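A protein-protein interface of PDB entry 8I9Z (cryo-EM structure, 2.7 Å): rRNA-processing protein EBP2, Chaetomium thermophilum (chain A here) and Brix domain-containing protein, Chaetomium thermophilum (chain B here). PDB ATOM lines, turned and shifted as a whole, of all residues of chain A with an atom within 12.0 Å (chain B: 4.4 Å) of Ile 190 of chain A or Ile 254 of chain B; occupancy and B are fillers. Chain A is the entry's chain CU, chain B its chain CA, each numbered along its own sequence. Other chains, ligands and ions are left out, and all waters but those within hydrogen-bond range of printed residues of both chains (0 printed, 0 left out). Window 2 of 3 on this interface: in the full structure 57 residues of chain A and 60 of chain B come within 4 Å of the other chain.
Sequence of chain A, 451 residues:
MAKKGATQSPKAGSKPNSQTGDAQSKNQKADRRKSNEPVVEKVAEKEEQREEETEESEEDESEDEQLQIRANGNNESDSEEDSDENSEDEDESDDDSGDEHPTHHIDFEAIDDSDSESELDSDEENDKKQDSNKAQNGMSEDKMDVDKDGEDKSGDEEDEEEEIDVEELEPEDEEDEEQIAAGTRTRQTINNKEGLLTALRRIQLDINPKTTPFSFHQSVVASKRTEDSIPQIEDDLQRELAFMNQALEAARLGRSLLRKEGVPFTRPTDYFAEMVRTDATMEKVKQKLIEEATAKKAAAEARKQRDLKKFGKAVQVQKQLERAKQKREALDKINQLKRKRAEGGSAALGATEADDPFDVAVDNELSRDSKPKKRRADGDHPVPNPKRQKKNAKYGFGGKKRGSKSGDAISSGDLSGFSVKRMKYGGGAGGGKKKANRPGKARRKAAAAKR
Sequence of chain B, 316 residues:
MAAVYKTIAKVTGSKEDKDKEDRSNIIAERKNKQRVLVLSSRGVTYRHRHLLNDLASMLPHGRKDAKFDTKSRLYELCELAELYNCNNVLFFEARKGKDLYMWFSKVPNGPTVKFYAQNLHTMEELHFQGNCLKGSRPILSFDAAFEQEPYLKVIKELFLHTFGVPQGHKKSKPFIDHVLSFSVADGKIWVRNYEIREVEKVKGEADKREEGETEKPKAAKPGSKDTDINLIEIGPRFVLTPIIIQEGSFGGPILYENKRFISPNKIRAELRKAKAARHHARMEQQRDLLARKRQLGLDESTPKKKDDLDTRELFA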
ATOM      1  N   ILE A 190      -0.752  27.975 -23.683  1.00  0.00           N
ATOM      2  CA  ILE A 190      -1.374  27.248 -22.585  1.00  0.00           C
ATOM      3  C   ILE A 190      -1.343  28.081 -21.310  1.00  0.00           C
ATOM      4  O   ILE A 190      -0.281  28.327 -20.745  1.00  0.00           O
ATOM      5  CB  ILE A 190      -0.687  25.893 -22.357  1.00  0.00           C
ATOM      6  CG1 ILE A 190      -0.800  25.019 -23.604  1.00  0.00           C
ATOM      7  CG2 ILE A 190      -1.310  25.183 -21.175  1.00  0.00           C
ATOM      8  CD1 ILE A 190      -0.181  23.647 -23.447  1.00  0.00           C
ATOM      9  N   ASN A 191      -2.518  28.528 -20.869  1.00  0.00           N
ATOM     10  CA  ASN A 191      -2.666  29.246 -19.604  1.00  0.00           C
ATOM     11  C   ASN A 191      -3.988  28.801 -18.994  1.00  0.00           C
ATOM     12  O   ASN A 191      -5.041  29.367 -19.301  1.00  0.00           O
ATOM     13  CB  ASN A 191      -2.627  30.755 -19.805  1.00  0.00           C
ATOM     14  CG  ASN A 191      -2.324  31.507 -18.526  1.00  0.00           C
ATOM     15  OD1 ASN A 191      -2.343  30.937 -17.436  1.00  0.00           O
ATOM     16  ND2 ASN A 191      -2.047  32.796 -18.651  1.00  0.00           N
ATOM     17  N   ASN A 192      -3.933  27.792 -18.136  1.00  0.00           N
ATOM     18  CA  ASN A 192      -5.124  27.222 -17.513  1.00  0.00           C
ATOM     19  C   ASN A 192      -5.377  27.986 -16.221  1.00  0.00           C
ATOM     20  O   ASN A 192      -4.841  27.655 -15.164  1.00  0.00           O
ATOM     21  CB  ASN A 192      -4.948  25.729 -17.273  1.00  0.00           C
ATOM     22  CG  ASN A 192      -6.264  25.005 -17.162  1.00  0.00           C
ATOM     23  OD1 ASN A 192      -7.322  25.626 -17.123  1.00  0.00           O
ATOM     24  ND2 ASN A 192      -6.209  23.683 -17.122  1.00  0.00           N
ATOM     25  N   LYS A 193      -6.217  29.019 -16.314  1.00  0.00           N
ATOM     26  CA  LYS A 193      -6.454  29.892 -15.170  1.00  0.00           C
ATOM     27  C   LYS A 193      -7.276  29.194 -14.096  1.00  0.00           C
ATOM     28  O   LYS A 193      -7.075  29.436 -12.902  1.00  0.00           O
ATOM     29  CB  LYS A 193      -7.139  31.173 -15.629  1.00  0.00           C
ATOM     30  CG  LYS A 193      -6.166  32.292 -15.931  1.00  0.00           C
ATOM     31  CD  LYS A 193      -6.865  33.500 -16.510  1.00  0.00           C
ATOM     32  CE  LYS A 193      -6.087  34.069 -17.676  1.00  0.00           C
ATOM     33  NZ  LYS A 193      -5.820  35.521 -17.495  1.00  0.00           N
ATOM     34  N   GLU A 194      -8.212  28.336 -14.497  1.00  0.00           N
ATOM     35  CA  GLU A 194      -8.984  27.583 -13.516  1.00  0.00           C
ATOM     36  C   GLU A 194      -8.137  26.501 -12.865  1.00  0.00           C
ATOM     37  O   GLU A 194      -8.275  26.229 -11.668  1.00  0.00           O
ATOM     38  CB  GLU A 194     -10.219  26.971 -14.174  1.00  0.00           C
ATOM     39  CG  GLU A 194     -11.032  27.957 -14.994  1.00  0.00           C
ATOM     40  CD  GLU A 194     -11.292  27.464 -16.402  1.00  0.00           C
ATOM     41  OE1 GLU A 194     -11.181  26.242 -16.636  1.00  0.00           O
ATOM     42  OE2 GLU A 194     -11.604  28.299 -17.277  1.00  0.00           O
ATOM     43  N   GLY A 195      -7.265  25.863 -13.646  1.00  0.00           N
ATOM     44  CA  GLY A 195      -6.410  24.826 -13.094  1.00  0.00           C
ATOM     45  C   GLY A 195      -5.374  25.369 -12.131  1.00  0.00           C
ATOM     46  O   GLY A 195      -5.046  24.724 -11.132  1.00  0.00           O
ATOM     47  N   LEU A 196      -4.834  26.552 -12.425  1.00  0.00           N
ATOM     48  CA  LEU A 196      -3.804  27.132 -11.569  1.00  0.00           C
ATOM     49  C   LEU A 196      -4.374  27.563 -10.225  1.00  0.00           C
ATOM     50  O   LEU A 196      -3.696  27.462  -9.198  1.00  0.00           O
ATOM     51  CB  LEU A 196      -3.137  28.311 -12.276  1.00  0.00           C
ATOM     52  CG  LEU A 196      -2.072  27.933 -13.300  1.00  0.00           C
ATOM     53  CD1 LEU A 196      -1.906  29.026 -14.333  1.00  0.00           C
ATOM     54  CD2 LEU A 196      -0.755  27.647 -12.615  1.00  0.00           C
ATOM     55  N   LEU A 197      -5.614  28.054 -10.214  1.00  0.00           N
ATOM     56  CA  LEU A 197      -6.255  28.411  -8.955  1.00  0.00           C
ATOM     57  C   LEU A 197      -6.540  27.178  -8.110  1.00  0.00           C
ATOM     58  O   LEU A 197      -6.367  27.204  -6.887  1.00  0.00           O
ATOM     59  CB  LEU A 197      -7.542  29.189  -9.225  1.00  0.00           C
ATOM     60  CG  LEU A 197      -7.426  30.619  -9.758  1.00  0.00           C
ATOM     61  CD1 LEU A 197      -8.632  31.436  -9.333  1.00  0.00           C
ATOM     62  CD2 LEU A 197      -6.144  31.295  -9.299  1.00  0.00           C
ATOM     63  N   THR A 198      -6.984  26.089  -8.743  1.00  0.00           N
ATOM     64  CA  THR A 198      -7.213  24.848  -8.009  1.00  0.00           C
ATOM     65  C   THR A 198      -5.902  24.244  -7.523  1.00  0.00           C
ATOM     66  O   THR A 198      -5.863  23.603  -6.468  1.00  0.00           O
ATOM     67  CB  THR A 198      -7.966  23.847  -8.878  1.00  0.00           C
ATOM     68  OG1 THR A 198      -7.288  23.693 -10.128  1.00  0.00           O
ATOM     69  CG2 THR A 198      -9.381  24.327  -9.133  1.00  0.00           C
ATOM     70  N   ALA A 199      -4.823  24.428  -8.285  1.00  0.00           N
ATOM     71  CA  ALA A 199      -3.509  24.012  -7.813  1.00  0.00           C
ATOM     72  C   ALA A 199      -3.070  24.848  -6.620  1.00  0.00           C
ATOM     73  O   ALA A 199      -2.374  24.352  -5.725  1.00  0.00           O
ATOM     74  CB  ALA A 199      -2.488  24.110  -8.945  1.00  0.00           C
ATOM     75  N   ARG A 202      -5.165  23.888  -3.241  1.00  0.00           N
ATOM     76  CA  ARG A 202      -4.819  22.610  -2.637  1.00  0.00           C
ATOM     77  C   ARG A 202      -3.583  22.715  -1.754  1.00  0.00           C
ATOM     78  O   ARG A 202      -3.352  21.836  -0.917  1.00  0.00           O
ATOM     79  CB  ARG A 202      -4.620  21.561  -3.730  1.00  0.00           C
ATOM     80  CG  ARG A 202      -5.180  20.200  -3.376  1.00  0.00           C
ATOM     81  CD  ARG A 202      -5.615  19.420  -4.607  1.00  0.00           C
ATOM     82  NE  ARG A 202      -4.882  19.806  -5.806  1.00  0.00           N
ATOM     83  CZ  ARG A 202      -5.392  19.794  -7.029  1.00  0.00           C
ATOM     84  NH1 ARG A 202      -6.637  19.410  -7.255  1.00  0.00           N
ATOM     85  NH2 ARG A 202      -4.633  20.170  -8.053  1.00  0.00           N
ATOM     86  N   ILE B 244       7.449  26.673 -17.247  1.00  0.00           N
ATOM     87  CA  ILE B 244       6.281  25.802 -17.197  1.00  0.00           C
ATOM     88  C   ILE B 244       5.837  25.619 -15.753  1.00  0.00           C
ATOM     89  O   ILE B 244       6.617  25.798 -14.818  1.00  0.00           O
ATOM     90  CB  ILE B 244       6.583  24.452 -17.899  1.00  0.00           C
ATOM     91  CG1 ILE B 244       5.354  23.997 -18.657  1.00  0.00           C
ATOM     92  CG2 ILE B 244       7.046  23.386 -16.917  1.00  0.00           C
ATOM     93  CD1 ILE B 244       5.642  23.059 -19.732  1.00  0.00           C
ATOM     94  N   ILE B 245       4.556  25.300 -15.573  1.00  0.00           N
ATOM     95  CA  ILE B 245       3.965  24.969 -14.280  1.00  0.00           C
ATOM     96  C   ILE B 245       3.206  23.660 -14.445  1.00  0.00           C
ATOM     97  O   ILE B 245       2.300  23.567 -15.281  1.00  0.00           O
ATOM     98  CB  ILE B 245       3.019  26.069 -13.768  1.00  0.00           C
ATOM     99  CG1 ILE B 245       3.754  27.398 -13.588  1.00  0.00           C
ATOM    100  CG2 ILE B 245       2.373  25.635 -12.471  1.00  0.00           C
ATOM    101  CD1 ILE B 245       2.936  28.463 -12.900  1.00  0.00           C
ATOM    102  N   GLN B 246       3.563  22.658 -13.650  1.00  0.00           N
ATOM    103  CA  GLN B 246       2.965  21.334 -13.714  1.00  0.00           C
ATOM    104  C   GLN B 246       1.968  21.151 -12.579  1.00  0.00           C
ATOM    105  O   GLN B 246       2.101  21.733 -11.502  1.00  0.00           O
ATOM    106  CB  GLN B 246       4.042  20.246 -13.639  1.00  0.00           C
ATOM    107  CG  GLN B 246       4.369  19.603 -14.963  1.00  0.00           C
ATOM    108  CD  GLN B 246       5.806  19.144 -15.045  1.00  0.00           C
ATOM    109  OE1 GLN B 246       6.596  19.377 -14.135  1.00  0.00           O
ATOM    110  NE2 GLN B 246       6.154  18.487 -16.145  1.00  0.00           N
ATOM    111  N   GLY B 252       3.112  15.756 -15.111  1.00  0.00           N
ATOM    112  CA  GLY B 252       1.677  15.825 -15.041  1.00  0.00           C
ATOM    113  C   GLY B 252       1.151  16.795 -16.071  1.00  0.00           C
ATOM    114  O   GLY B 252       1.871  17.203 -16.986  1.00  0.00           O
ATOM    115  N   PRO B 253      -0.118  17.172 -15.953  1.00  0.00           N
ATOM    116  CA  PRO B 253      -0.698  18.116 -16.912  1.00  0.00           C
ATOM    117  C   PRO B 253      -0.051  19.487 -16.805  1.00  0.00           C
ATOM    118  O   PRO B 253       0.406  19.901 -15.739  1.00  0.00           O
ATOM    119  CB  PRO B 253      -2.177  18.150 -16.519  1.00  0.00           C
ATOM    120  CG  PRO B 253      -2.396  16.862 -15.831  1.00  0.00           C
ATOM    121  CD  PRO B 253      -1.143  16.591 -15.077  1.00  0.00           C
ATOM    122  N   ILE B 254      -0.006  20.188 -17.929  1.00  0.00           N
ATOM    123  CA  ILE B 254       0.639  21.488 -18.023  1.00  0.00           C
ATOM    124  C   ILE B 254      -0.423  22.556 -17.837  1.00  0.00           C
ATOM    125  O   ILE B 254      -1.373  22.644 -18.623  1.00  0.00           O
ATOM    126  CB  ILE B 254       1.365  21.655 -19.365  1.00  0.00           C
ATOM    127  CG1 ILE B 254       2.442  20.583 -19.513  1.00  0.00           C
ATOM    128  CG2 ILE B 254       1.931  23.045 -19.494  1.00  0.00           C
ATOM    129  CD1 ILE B 254       3.419  20.545 -18.383  1.00  0.00           C
ATOM    130  N   LEU B 255      -0.269  23.366 -16.797  1.00  0.00           N
ATOM    131  CA  LEU B 255      -1.228  24.422 -16.519  1.00  0.00           C
ATOM    132  C   LEU B 255      -0.820  25.742 -17.153  1.00  0.00           C
ATOM    133  O   LEU B 255      -1.683  26.504 -17.601  1.00  0.00           O
ATOM    134  CB  LEU B 255      -1.394  24.583 -15.009  1.00  0.00           C
ATOM    135  CG  LEU B 255      -1.749  23.276 -14.302  1.00  0.00           C
ATOM    136  CD1 LEU B 255      -1.787  23.471 -12.803  1.00  0.00           C
ATOM    137  CD2 LEU B 255      -3.073  22.739 -14.804  1.00  0.00           C
ATOM    138  N   TYR B 256       0.478  26.030 -17.204  1.00  0.00           N
ATOM    139  CA  TYR B 256       0.976  27.243 -17.831  1.00  0.00           C
ATOM    140  C   TYR B 256       2.217  26.925 -18.649  1.00  0.00           C
ATOM    141  O   TYR B 256       3.086  26.179 -18.200  1.00  0.00           O
ATOM    142  CB  TYR B 256       1.318  28.316 -16.796  1.00  0.00           C
ATOM    143  CG  TYR B 256       1.907  29.562 -17.407  1.00  0.00           C
ATOM    144  CD1 TYR B 256       1.128  30.408 -18.180  1.00  0.00           C
ATOM    145  CD2 TYR B 256       3.243  29.880 -17.231  1.00  0.00           C
ATOM    146  CE1 TYR B 256       1.661  31.545 -18.748  1.00  0.00           C
ATOM    147  CE2 TYR B 256       3.785  31.010 -17.797  1.00  0.00           C
ATOM    148  CZ  TYR B 256       2.989  31.839 -18.552  1.00  0.00           C
ATOM    149  OH  TYR B 256       3.525  32.969 -19.118  1.00  0.00           O
ATOM    150  N   GLU B 257       2.292  27.501 -19.847  1.00  0.00           N
ATOM    151  CA  GLU B 257       3.468  27.425 -20.699  1.00  0.00           C
ATOM    152  C   GLU B 257       3.861  28.835 -21.104  1.00  0.00           C
ATOM    153  O   GLU B 257       2.991  29.685 -21.317  1.00  0.00           O
ATOM    154  CB  GLU B 257       3.208  26.573 -21.944  1.00  0.00           C
ATOM    155  CG  GLU B 257       4.322  25.601 -22.275  1.00  0.00           C
ATOM    156  CD  GLU B 257       4.311  25.189 -23.731  1.00  0.00           C
ATOM    157  OE1 GLU B 257       3.258  25.336 -24.382  1.00  0.00           O
ATOM    158  OE2 GLU B 257       5.358  24.729 -24.229  1.00  0.00           O
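The backbone carbonyl oxygen (O) of Ile 190 of chain A is in hydrogen-bond range of the backbone NH (N) of Glu 257 of chain B (2.8 Å). The backbone carbonyl oxygen of Leu 255 of chain B is in hydrogen-bond range of the backbone NH of Asn 192 of chain A, at 2.6 Å.
OD1 of Asn 192 of chain A sits at hydrogen-bond distance from N of Gly 195 of chain A (3.5 Å). The backbone carbonyl oxygen (O) of Gly 195 of chain A is in hydrogen-bond range of the side-chain hydroxyl (OG1) of Thr 198 of chain A (2.7 Å). The backbone NH of Leu 255 of chain B lies within hydrogen-bond range of the backbone carbonyl oxygen of Ile 245 of chain B. N of Ile 245 of chain B is in hydrogen-bond range of O of Tyr 256 of chain B (3.1 Å).
Among the printed residues, pairs that only touch across the chains: Ile 190 of chain A with Tyr 256 of chain B, Asn 191 of chain A with Leu 255 of chain B, Asn 191 of chain A with Tyr 256 of chain B, Ile 190 of chain A with Ile 254 of chain B, Leu 196 of chain A with Ile 245 of chain B, Leu 196 of chain A with Leu 255 of chain B, Ile 190 of chain A with Leu 255 of chain B, Gly 195 of chain A with Leu 255 of chain B and Ala 199 of chain A with Leu 255 of chain B.
Of the printed residues of chain B, Ile 190 of chain A touches Ile 254, Leu 255, Tyr 256 and Glu 257. Printed residues of chain B within 4 Å of Asn 191 of chain A: Leu 255 and Tyr 256. Of the printed residues of chain B, Gly 195 of chain A touches Leu 255. Leu 197 of chain A touches none of the printed residues of chain B. Of the printed residues of chain B, Ala 199 of chain A touches Leu 255. Of the printed residues of chain A, Ile 245 of chain B touches Leu 196 (3.7 Å). Gln 246 of chain B touches none of the printed residues of chain A. No residue of chain A comes within 4 Å of Gly 252 of chain B. No residue of chain A comes within 4 Å of Pro 253 of chain B. Of the printed residues of chain A, Ile 254 of chain B touches Ile 190 (3.6 Å). Printed residues of chain A within 4 Å of Leu 255 of chain B: Ile 190 (3.8 Å), Asn 191 (3.5 Å), Asn 192 (2.6 Å), Gly 195 (3.9 Å), Leu 196 (3.8 Å) and Ala 199 (3.97 Å). The nearest residue of chain A that does not touch Ile 254 of chain B is Asn 192 of chain A (4.9 Å).
Of the 11 printed residues of chain A, 6 touch a printed residue of chain B. Hydrophobic or aromatic side chains of chain A that line the printed part of chain B: Ile 190, Leu 196 and Ala 199. Of the 9 printed residues of chain B, 5 touch a printed residue of chain A. Among the printed residues, 11 pairs touch across the chains.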
